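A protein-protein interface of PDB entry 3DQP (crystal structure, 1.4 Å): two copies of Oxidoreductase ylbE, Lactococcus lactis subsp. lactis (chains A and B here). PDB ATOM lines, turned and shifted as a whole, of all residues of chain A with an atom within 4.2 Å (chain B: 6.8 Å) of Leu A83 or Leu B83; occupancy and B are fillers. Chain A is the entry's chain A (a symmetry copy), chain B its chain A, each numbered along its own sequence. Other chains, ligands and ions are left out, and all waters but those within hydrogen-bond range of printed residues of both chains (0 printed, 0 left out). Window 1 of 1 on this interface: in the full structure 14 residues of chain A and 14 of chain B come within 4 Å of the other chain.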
ATOM      1  N   LEU A  78     -28.930 -21.703   7.919  1.00  0.00           N
ATOM      2  CA  LEU A  78     -28.927 -20.951   9.173  1.00  0.00           C
ATOM      3  C   LEU A  78     -28.123 -19.657   9.137  1.00  0.00           C
ATOM      4  O   LEU A  78     -28.563 -18.635   9.673  1.00  0.00           O
ATOM      5  CB  LEU A  78     -28.444 -21.830  10.328  1.00  0.00           C
ATOM      6  CG  LEU A  78     -29.316 -23.039  10.662  1.00  0.00           C
ATOM      7  CD1 LEU A  78     -28.559 -23.962  11.578  1.00  0.00           C
ATOM      8  CD2 LEU A  78     -30.624 -22.596  11.314  1.00  0.00           C
ATOM      9  N   LEU A  79     -26.946 -19.695   8.516  1.00  0.00           N
ATOM     10  CA  LEU A  79     -26.120 -18.501   8.432  1.00  0.00           C
ATOM     11  C   LEU A  79     -26.745 -17.433   7.534  1.00  0.00           C
ATOM     12  O   LEU A  79     -26.783 -16.259   7.897  1.00  0.00           O
ATOM     13  CB  LEU A  79     -24.711 -18.853   7.963  1.00  0.00           C
ATOM     14  CG  LEU A  79     -23.821 -19.496   9.031  1.00  0.00           C
ATOM     15  CD1 LEU A  79     -22.673 -20.269   8.402  1.00  0.00           C
ATOM     16  CD2 LEU A  79     -23.275 -18.449   9.990  1.00  0.00           C
ATOM     17  N   VAL A  81     -30.039 -17.190   6.394  1.00  0.00           N
ATOM     18  CA  VAL A  81     -31.423 -16.783   6.660  1.00  0.00           C
ATOM     19  C   VAL A  81     -31.635 -16.393   8.126  1.00  0.00           C
ATOM     20  O   VAL A  81     -31.928 -15.234   8.430  1.00  0.00           O
ATOM     21  CB  VAL A  81     -32.439 -17.880   6.235  1.00  0.00           C
ATOM     22  CG1 VAL A  81     -33.857 -17.488   6.635  1.00  0.00           C
ATOM     23  CG2 VAL A  81     -32.366 -18.147   4.729  1.00  0.00           C
ATOM     24  N   ASP A  82     -31.445 -17.350   9.032  1.00  0.00           N
ATOM     25  CA  ASP A  82     -31.783 -17.153  10.445  1.00  0.00           C
ATOM     26  C   ASP A  82     -30.883 -16.153  11.167  1.00  0.00           C
ATOM     27  O   ASP A  82     -31.310 -15.499  12.125  1.00  0.00           O
ATOM     28  CB  ASP A  82     -31.803 -18.488  11.192  1.00  0.00           C
ATOM     29  CG  ASP A  82     -32.619 -19.540  10.474  1.00  0.00           C
ATOM     30  OD1 ASP A  82     -32.178 -19.982   9.390  1.00  0.00           O
ATOM     31  OD2 ASP A  82     -33.690 -19.924  11.000  1.00  0.00           O
ATOM     32  N   LEU A  83     -29.639 -16.041  10.705  1.00  0.00           N
ATOM     33  CA  LEU A  83     -28.724 -15.057  11.263  1.00  0.00           C
ATOM     34  C   LEU A  83     -28.597 -13.814  10.376  1.00  0.00           C
ATOM     35  O   LEU A  83     -29.096 -12.748  10.730  1.00  0.00           O
ATOM     36  CB  LEU A  83     -27.351 -15.683  11.553  1.00  0.00           C
ATOM     37  CG  LEU A  83     -26.240 -14.733  12.022  1.00  0.00           C
ATOM     38  CD1 LEU A  83     -26.685 -13.862  13.210  1.00  0.00           C
ATOM     39  CD2 LEU A  83     -24.983 -15.523  12.345  1.00  0.00           C
ATOM     40  N   TYR A  84     -27.948 -13.957   9.223  1.00  0.00           N
ATOM     41  CA  TYR A  84     -27.629 -12.800   8.394  1.00  0.00           C
ATOM     42  C   TYR A  84     -28.883 -12.122   7.842  1.00  0.00           C
ATOM     43  O   TYR A  84     -29.014 -10.904   7.918  1.00  0.00           O
ATOM     44  CB  TYR A  84     -26.682 -13.225   7.275  1.00  0.00           C
ATOM     45  CG  TYR A  84     -26.042 -12.120   6.466  1.00  0.00           C
ATOM     46  CD1 TYR A  84     -25.898 -12.267   5.090  1.00  0.00           C
ATOM     47  CD2 TYR A  84     -25.564 -10.951   7.055  1.00  0.00           C
ATOM     48  CE1 TYR A  84     -25.295 -11.294   4.312  1.00  0.00           C
ATOM     49  CE2 TYR A  84     -24.953  -9.947   6.266  1.00  0.00           C
ATOM     50  CZ  TYR A  84     -24.829 -10.144   4.897  1.00  0.00           C
ATOM     51  OH  TYR A  84     -24.239  -9.199   4.078  1.00  0.00           O
ATOM     52  N   GLY A  85     -29.816 -12.912   7.322  1.00  0.00           N
ATOM     53  CA  GLY A  85     -31.079 -12.357   6.822  1.00  0.00           C
ATOM     54  C   GLY A  85     -31.816 -11.558   7.885  1.00  0.00           C
ATOM     55  O   GLY A  85     -32.298 -10.451   7.625  1.00  0.00           O
ATOM     56  N   ALA A  86     -31.889 -12.113   9.091  1.00  0.00           N
ATOM     57  CA  ALA A  86     -32.557 -11.460  10.211  1.00  0.00           C
ATOM     58  C   ALA A  86     -31.879 -10.138  10.567  1.00  0.00           C
ATOM     59  O   ALA A  86     -32.542  -9.122  10.770  1.00  0.00           O
ATOM     60  CB  ALA A  86     -32.592 -12.385  11.418  1.00  0.00           C
ATOM     61  N   VAL A  87     -30.554 -10.156  10.635  1.00  0.00           N
ATOM     62  CA  VAL A  87     -29.799  -8.951  10.943  1.00  0.00           C
ATOM     63  C   VAL A  87     -29.926  -7.890   9.839  1.00  0.00           C
ATOM     64  O   VAL A  87     -30.113  -6.710  10.133  1.00  0.00           O
ATOM     65  CB  VAL A  87     -28.324  -9.288  11.261  1.00  0.00           C
ATOM     66  CG1 VAL A  87     -27.476  -8.025  11.345  1.00  0.00           C
ATOM     67  CG2 VAL A  87     -28.253 -10.081  12.563  1.00  0.00           C
ATOM     68  N   ALA A 129     -27.173 -19.521  15.624  1.00  0.00           N
ATOM     69  CA  ALA A 129     -27.677 -18.536  14.672  1.00  0.00           C
ATOM     70  C   ALA A 129     -28.669 -17.576  15.327  1.00  0.00           C
ATOM     71  O   ALA A 129     -28.541 -16.355  15.194  1.00  0.00           O
ATOM     72  CB  ALA A 129     -28.288 -19.221  13.457  1.00  0.00           C
ATOM     73  N   PHE A 132     -26.996 -15.081  18.020  1.00  0.00           N
ATOM     74  CA  PHE A 132     -26.290 -13.920  17.497  1.00  0.00           C
ATOM     75  C   PHE A 132     -27.206 -12.875  16.871  1.00  0.00           C
ATOM     76  O   PHE A 132     -26.945 -11.679  16.986  1.00  0.00           O
ATOM     77  CB  PHE A 132     -25.146 -14.341  16.571  1.00  0.00           C
ATOM     78  CG  PHE A 132     -23.928 -14.786  17.329  1.00  0.00           C
ATOM     79  CD1 PHE A 132     -23.045 -13.845  17.842  1.00  0.00           C
ATOM     80  CD2 PHE A 132     -23.710 -16.131  17.612  1.00  0.00           C
ATOM     81  CE1 PHE A 132     -21.943 -14.238  18.585  1.00  0.00           C
ATOM     82  CE2 PHE A 132     -22.599 -16.528  18.359  1.00  0.00           C
ATOM     83  CZ  PHE A 132     -21.719 -15.575  18.845  1.00  0.00           C
ATOM     84  N   ALA A 133     -28.301 -13.310  16.255  1.00  0.00           N
ATOM     85  CA  ALA A 133     -29.303 -12.353  15.771  1.00  0.00           C
ATOM     86  C   ALA A 133     -29.980 -11.608  16.926  1.00  0.00           C
ATOM     87  O   ALA A 133     -30.226 -10.407  16.827  1.00  0.00           O
ATOM     88  CB  ALA A 133     -30.329 -13.038  14.917  1.00  0.00           C
ATOM     89  N   SER B  77     -17.909 -26.687  10.056  1.00  0.00           N
ATOM     90  CA  SER B  77     -18.625 -26.429  11.308  1.00  0.00           C
ATOM     91  C   SER B  77     -18.561 -24.938  11.644  1.00  0.00           C
ATOM     92  O   SER B  77     -18.025 -24.535  12.671  1.00  0.00           O
ATOM     93  CB  SER B  77     -18.063 -27.287  12.446  1.00  0.00           C
ATOM     94  OG  SER B  77     -19.020 -27.432  13.478  1.00  0.00           O
ATOM     95  N   LEU B  78     -19.133 -24.130  10.758  1.00  0.00           N
ATOM     96  CA  LEU B  78     -18.969 -22.677  10.809  1.00  0.00           C
ATOM     97  C   LEU B  78     -19.623 -22.004  12.009  1.00  0.00           C
ATOM     98  O   LEU B  78     -19.036 -21.101  12.613  1.00  0.00           O
ATOM     99  CB  LEU B  78     -19.470 -22.033   9.515  1.00  0.00           C
ATOM    100  CG  LEU B  78     -18.718 -22.413   8.241  1.00  0.00           C
ATOM    101  CD1 LEU B  78     -19.511 -21.967   7.042  1.00  0.00           C
ATOM    102  CD2 LEU B  78     -17.328 -21.780   8.225  1.00  0.00           C
ATOM    103  N   LEU B  79     -20.836 -22.432  12.354  1.00  0.00           N
ATOM    104  CA  LEU B  79     -21.526 -21.846  13.492  1.00  0.00           C
ATOM    105  C   LEU B  79     -20.846 -22.193  14.817  1.00  0.00           C
ATOM    106  O   LEU B  79     -20.653 -21.323  15.663  1.00  0.00           O
ATOM    107  CB  LEU B  79     -22.993 -22.264  13.505  1.00  0.00           C
ATOM    108  CG  LEU B  79     -23.877 -21.537  12.486  1.00  0.00           C
ATOM    109  CD1 LEU B  79     -25.143 -22.325  12.192  1.00  0.00           C
ATOM    110  CD2 LEU B  79     -24.237 -20.141  12.973  1.00  0.00           C
ATOM    111  N   LYS B  80     -20.477 -23.460  14.983  1.00  0.00           N
ATOM    112  CA  LYS B  80     -19.865 -23.925  16.230  1.00  0.00           C
ATOM    113  C   LYS B  80     -18.428 -23.437  16.428  1.00  0.00           C
ATOM    114  O   LYS B  80     -18.051 -23.055  17.538  1.00  0.00           O
ATOM    115  CB  LYS B  80     -19.926 -25.452  16.331  1.00  0.00           C
ATOM    116  CG  LYS B  80     -21.321 -25.981  16.664  1.00  0.00           C
ATOM    117  CD  LYS B  80     -21.414 -27.485  16.428  1.00  0.00           C
ATOM    118  CE  LYS B  80     -22.801 -28.016  16.771  1.00  0.00           C
ATOM    119  NZ  LYS B  80     -22.973 -29.427  16.309  1.00  0.00           N
ATOM    120  N   VAL B  81     -17.628 -23.442  15.361  1.00  0.00           N
ATOM    121  CA  VAL B  81     -16.193 -23.173  15.495  1.00  0.00           C
ATOM    122  C   VAL B  81     -15.842 -21.732  15.113  1.00  0.00           C
ATOM    123  O   VAL B  81     -15.400 -20.948  15.958  1.00  0.00           O
ATOM    124  CB  VAL B  81     -15.337 -24.178  14.676  1.00  0.00           C
ATOM    125  CG1 VAL B  81     -13.861 -23.802  14.731  1.00  0.00           C
ATOM    126  CG2 VAL B  81     -15.540 -25.612  15.176  1.00  0.00           C
ATOM    127  N   ASP B  82     -16.077 -21.374  13.852  1.00  0.00           N
ATOM    128  CA  ASP B  82     -15.626 -20.084  13.320  1.00  0.00           C
ATOM    129  C   ASP B  82     -16.358 -18.878  13.903  1.00  0.00           C
ATOM    130  O   ASP B  82     -15.797 -17.780  13.983  1.00  0.00           O
ATOM    131  CB  ASP B  82     -15.706 -20.068  11.791  1.00  0.00           C
ATOM    132  CG  ASP B  82     -15.063 -21.286  11.166  1.00  0.00           C
ATOM    133  OD1 ASP B  82     -15.622 -22.393  11.333  1.00  0.00           O
ATOM    134  OD2 ASP B  82     -14.009 -21.129  10.505  1.00  0.00           O
ATOM    135  N   LEU B  83     -17.609 -19.089  14.307  1.00  0.00           N
ATOM    136  CA  LEU B  83     -18.369 -18.032  14.956  1.00  0.00           C
ATOM    137  C   LEU B  83     -18.415 -18.202  16.479  1.00  0.00           C
ATOM    138  O   LEU B  83     -17.776 -17.442  17.205  1.00  0.00           O
ATOM    139  CB  LEU B  83     -19.781 -17.921  14.361  1.00  0.00           C
ATOM    140  CG  LEU B  83     -20.745 -16.936  15.038  1.00  0.00           C
ATOM    141  CD1 LEU B  83     -20.127 -15.535  15.194  1.00  0.00           C
ATOM    142  CD2 LEU B  83     -22.058 -16.888  14.276  1.00  0.00           C
ATOM    143  N   TYR B  84     -19.150 -19.203  16.955  1.00  0.00           N
ATOM    144  CA  TYR B  84     -19.392 -19.342  18.387  1.00  0.00           C
ATOM    145  C   TYR B  84     -18.109 -19.642  19.162  1.00  0.00           C
ATOM    146  O   TYR B  84     -17.837 -19.012  20.180  1.00  0.00           O
ATOM    147  CB  TYR B  84     -20.453 -20.414  18.619  1.00  0.00           C
ATOM    148  CG  TYR B  84     -21.017 -20.524  20.017  1.00  0.00           C
ATOM    149  CD1 TYR B  84     -21.268 -21.779  20.563  1.00  0.00           C
ATOM    150  CD2 TYR B  84     -21.321 -19.401  20.785  1.00  0.00           C
ATOM    151  CE1 TYR B  84     -21.808 -21.928  21.829  1.00  0.00           C
ATOM    152  CE2 TYR B  84     -21.866 -19.544  22.083  1.00  0.00           C
ATOM    153  CZ  TYR B  84     -22.102 -20.819  22.581  1.00  0.00           C
ATOM    154  OH  TYR B  84     -22.636 -21.018  23.841  1.00  0.00           O
ATOM    155  N   GLY B  85     -17.308 -20.576  18.661  1.00  0.00           N
ATOM    156  CA  GLY B  85     -16.026 -20.891  19.304  1.00  0.00           C
ATOM    157  C   GLY B  85     -15.135 -19.667  19.439  1.00  0.00           C
ATOM    158  O   GLY B  85     -14.550 -19.422  20.498  1.00  0.00           O
ATOM    159  N   ALA B  86     -15.045 -18.886  18.366  1.00  0.00           N
ATOM    160  CA  ALA B  86     -14.235 -17.672  18.350  1.00  0.00           C
ATOM    161  C   ALA B  86     -14.734 -16.659  19.377  1.00  0.00           C
ATOM    162  O   ALA B  86     -13.950 -16.074  20.122  1.00  0.00           O
ATOM    163  CB  ALA B  86     -14.224 -17.062  16.957  1.00  0.00           C
ATOM    164  N   VAL B  87     -16.046 -16.459  19.417  1.00  0.00           N
ATOM    165  CA  VAL B  87     -16.639 -15.532  20.370  1.00  0.00           C
ATOM    166  C   VAL B  87     -16.467 -16.007  21.821  1.00  0.00           C
ATOM    167  O   VAL B  87     -16.130 -15.211  22.697  1.00  0.00           O
ATOM    168  CB  VAL B  87     -18.118 -15.250  20.020  1.00  0.00           C
ATOM    169  CG1 VAL B  87     -18.811 -14.481  21.138  1.00  0.00           C
ATOM    170  CG2 VAL B  87     -18.191 -14.482  18.704  1.00  0.00           C
ATOM    171  N   LYS B  88     -16.673 -17.298  22.069  1.00  0.00           N
ATOM    172  CA  LYS B  88     -16.482 -17.832  23.416  1.00  0.00           C
ATOM    173  C   LYS B  88     -15.040 -17.616  23.877  1.00  0.00           C
ATOM    174  O   LYS B  88     -14.799 -17.315  25.046  1.00  0.00           O
ATOM    175  CB  LYS B  88     -16.841 -19.314  23.485  1.00  0.00           C
ATOM    176  CG  LYS B  88     -18.331 -19.587  23.422  1.00  0.00           C
ATOM    177  CD  LYS B  88     -18.628 -21.052  23.683  1.00  0.00           C
ATOM    178  CE  LYS B  88     -18.182 -21.951  22.547  1.00  0.00           C
ATOM    179  NZ  LYS B  88     -18.396 -23.393  22.854  1.00  0.00           N
ATOM    180  N   MET B  90     -13.083 -15.123  23.041  1.00  0.00           N
ATOM    181  CA  MET B  90     -12.992 -13.715  23.424  1.00  0.00           C
ATOM    182  C   MET B  90     -13.545 -13.505  24.828  1.00  0.00           C
ATOM    183  O   MET B  90     -12.943 -12.810  25.646  1.00  0.00           O
ATOM    184  CB  MET B  90     -13.769 -12.847  22.438  1.00  0.00           C
ATOM    185  CG  MET B  90     -13.284 -12.966  21.005  1.00  0.00           C
ATOM    186  SD  MET B  90     -14.563 -12.151  19.786  1.00  0.00           S
ATOM    187  CE  MET B  90     -13.901 -12.925  18.125  1.00  0.00           C
ATOM    188  N   ILE B 128     -20.176 -14.994   6.472  1.00  0.00           N
ATOM    189  CA  ILE B 128     -21.150 -14.601   7.493  1.00  0.00           C
ATOM    190  C   ILE B 128     -20.623 -14.947   8.887  1.00  0.00           C
ATOM    191  O   ILE B 128     -20.655 -14.106   9.788  1.00  0.00           O
ATOM    192  CB  ILE B 128     -22.536 -15.229   7.241  1.00  0.00           C
ATOM    193  CG1 ILE B 128     -23.134 -14.674   5.946  1.00  0.00           C
ATOM    194  CG2 ILE B 128     -23.487 -14.960   8.424  1.00  0.00           C
ATOM    195  CD1 ILE B 128     -24.277 -15.486   5.391  1.00  0.00           C
ATOM    196  N   ALA B 129     -20.118 -16.170   9.056  1.00  0.00           N
ATOM    197  CA  ALA B 129     -19.571 -16.590  10.342  1.00  0.00           C
ATOM    198  C   ALA B 129     -18.436 -15.675  10.797  1.00  0.00           C
ATOM    199  O   ALA B 129     -18.435 -15.196  11.936  1.00  0.00           O
ATOM    200  CB  ALA B 129     -19.123 -18.045  10.290  1.00  0.00           C
ATOM    201  N   LYS B 130     -17.493 -15.397   9.894  1.00  0.00           N
ATOM    202  CA  LYS B 130     -16.345 -14.550  10.230  1.00  0.00           C
ATOM    203  C   LYS B 130     -16.773 -13.110  10.506  1.00  0.00           C
ATOM    204  O   LYS B 130     -16.254 -12.461  11.418  1.00  0.00           O
ATOM    205  CB  LYS B 130     -15.278 -14.589   9.120  1.00  0.00           C
ATOM    206  CG  LYS B 130     -14.720 -15.988   8.799  1.00  0.00           C
ATOM    207  CD  LYS B 130     -13.991 -16.638   9.983  1.00  0.00           C
ATOM    208  CE  LYS B 130     -12.661 -15.957  10.283  1.00  0.00           C
ATOM    209  NZ  LYS B 130     -11.995 -16.586  11.463  1.00  0.00           N
ATOM    210  N   HIS B 131     -17.725 -12.615   9.717  1.00  0.00           N
ATOM    211  CA  HIS B 131     -18.262 -11.269   9.897  1.00  0.00           C
ATOM    212  C   HIS B 131     -18.793 -11.040  11.312  1.00  0.00           C
ATOM    213  O   HIS B 131     -18.443 -10.061  11.966  1.00  0.00           O
ATOM    214  CB  HIS B 131     -19.377 -11.003   8.882  1.00  0.00           C
ATOM    215  CG  HIS B 131     -19.899  -9.605   8.925  1.00  0.00           C
ATOM    216  ND1 HIS B 131     -21.197  -9.296   9.271  1.00  0.00           N
ATOM    217  CD2 HIS B 131     -19.282  -8.425   8.684  1.00  0.00           C
ATOM    218  CE1 HIS B 131     -21.358  -7.983   9.226  1.00  0.00           C
ATOM    219  NE2 HIS B 131     -20.209  -7.433   8.881  1.00  0.00           N
ATOM    220  N   PHE B 132     -19.636 -11.951  11.785  1.00  0.00           N
ATOM    221  CA  PHE B 132     -20.240 -11.777  13.098  1.00  0.00           C
ATOM    222  C   PHE B 132     -19.256 -11.930  14.252  1.00  0.00           C
ATOM    223  O   PHE B 132     -19.373 -11.233  15.258  1.00  0.00           O
ATOM    224  CB  PHE B 132     -21.484 -12.656  13.254  1.00  0.00           C
ATOM    225  CG  PHE B 132     -22.690 -12.069  12.581  1.00  0.00           C
ATOM    226  CD1 PHE B 132     -23.426 -11.076  13.212  1.00  0.00           C
ATOM    227  CD2 PHE B 132     -23.039 -12.437  11.284  1.00  0.00           C
ATOM    228  CE1 PHE B 132     -24.513 -10.490  12.584  1.00  0.00           C
ATOM    229  CE2 PHE B 132     -24.135 -11.848  10.650  1.00  0.00           C
ATOM    230  CZ  PHE B 132     -24.868 -10.873  11.306  1.00  0.00           C
ATOM    231  N   ALA B 133     -18.260 -12.798  14.097  1.00  0.00           N
ATOM    232  CA  ALA B 133     -17.191 -12.878  15.100  1.00  0.00           C
ATOM    233  C   ALA B 133     -16.360 -11.592  15.147  1.00  0.00           C
ATOM    234  O   ALA B 133     -15.988 -11.136  16.226  1.00  0.00           O
ATOM    235  CB  ALA B 133     -16.308 -14.064  14.846  1.00  0.00           C
ATOM    236  N   ASP B 134     -16.088 -11.006  13.977  1.00  0.00           N
ATOM    237  CA  ASP B 134     -15.348  -9.737  13.918  1.00  0.00           C
ATOM    238  C   ASP B 134     -16.133  -8.558  14.474  1.00  0.00           C
ATOM    239  O   ASP B 134     -15.552  -7.669  15.101  1.00  0.00           O
ATOM    240  CB  ASP B 134     -14.889  -9.426  12.494  1.00  0.00           C
ATOM    241  CG  ASP B 134     -13.806 -10.369  12.012  1.00  0.00           C
ATOM    242  OD1 ASP B 134     -13.221 -11.108  12.828  1.00  0.00           O
ATOM    243  OD2 ASP B 134     -13.542 -10.373  10.798  1.00  0.00           O
ATOM    244  N   TYR B 136     -18.316  -8.886  16.878  1.00  0.00           N
ATOM    245  CA  TYR B 136     -18.247  -9.114  18.317  1.00  0.00           C
ATOM    246  C   TYR B 136     -16.938  -8.587  18.902  1.00  0.00           C
ATOM    247  O   TYR B 136     -16.946  -7.861  19.895  1.00  0.00           O
ATOM    248  CB  TYR B 136     -18.437 -10.598  18.658  1.00  0.00           C
ATOM    249  CG  TYR B 136     -18.828 -10.819  20.108  1.00  0.00           C
ATOM    250  CD1 TYR B 136     -17.866 -10.805  21.119  1.00  0.00           C
ATOM    251  CD2 TYR B 136     -20.159 -11.032  20.468  1.00  0.00           C
ATOM    252  CE1 TYR B 136     -18.214 -10.990  22.446  1.00  0.00           C
ATOM    253  CE2 TYR B 136     -20.516 -11.226  21.800  1.00  0.00           C
ATOM    254  CZ  TYR B 136     -19.536 -11.206  22.780  1.00  0.00           C
ATOM    255  OH  TYR B 136     -19.856 -11.389  24.107  1.00  0.00           O
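Among the printed residues, pairs that only touch across the chains: Leu A78 with Leu B79, Leu A79 with Leu B78, Leu A79 with Leu B79, Leu A79 with Ile B128, Leu A83 with Leu B83, Leu A83 with Phe B132, Tyr A84 with Ile B128, Tyr A84 with Phe B132, Val A87 with Phe B132, Phe A132 with Leu B83, Phe A132 with Tyr B84 and Phe A132 with Val B87.
Printed residues of chain B within 4 Å of Leu A78: Leu B79 (3.8 Å). Of the printed residues of chain B, Leu A79 touches Leu B78 (3.8 Å), Leu B79 (3.6 Å) and Ile B128 (3.6 Å). Leu A83 touches two residues of chain B. Of the printed residues of chain B, Val A87 touches Phe B132. Leu B83 touches two residues of chain A. Of the printed residues of chain A, Val B87 touches Phe A132 (3.7 Å). Lys B130 touches none of the printed residues of chain A. Printed residues of chain A within 4 Å of Phe B132: Leu A83 (3.8 Å), Tyr A84 (3.97 Å) and Val A87 (3.7 Å).
Leu A78 touches Leu B79, and with the chains exchanged Leu A79 touches Leu B78. Leu B79 touches its own counterpart, Leu A79. Leu B83 touches its own counterpart, Leu A83. Leu A83 touches Phe B132, and with the chains exchanged Phe A132 touches Leu B83. Of the 12 pairs that touch across the chains among the printed residues, 10 have their exchanged pair printed and touching as well.
The backbone NH (N) of Tyr A84 lies within hydrogen-bond range of the backbone carbonyl oxygen (O) of Leu A79 (2.9 Å). The backbone carbonyl oxygen of Leu B78 lies within hydrogen-bond range of the backbone NH of Leu B83 (3.0 Å). The backbone carbonyl oxygen (O) of Leu B79 sits at hydrogen-bond distance from the backbone NH (N) of Tyr B84 (2.9 Å). O of Leu A78 sits at hydrogen-bond distance from N of Leu A83 (3.0 Å).
Of the 21 printed residues of chain B, 7 touch a printed residue of chain A. Hydrophobic or aromatic side chains of chain B within 4 Å of the printed part of chain A: Leu B78, Leu B79, Leu B83, Tyr B84, Val B87, Ile B128 and Phe B132. Printed residues of chain A that touch a printed residue of chain B: Leu A78, Leu A79, Leu A83, Tyr A84, Val A87 and Phe A132. Among the printed residues, no Asp or Glu carboxylate lies within 4 Å of a Lys or Arg side-chain nitrogen of the other chain.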
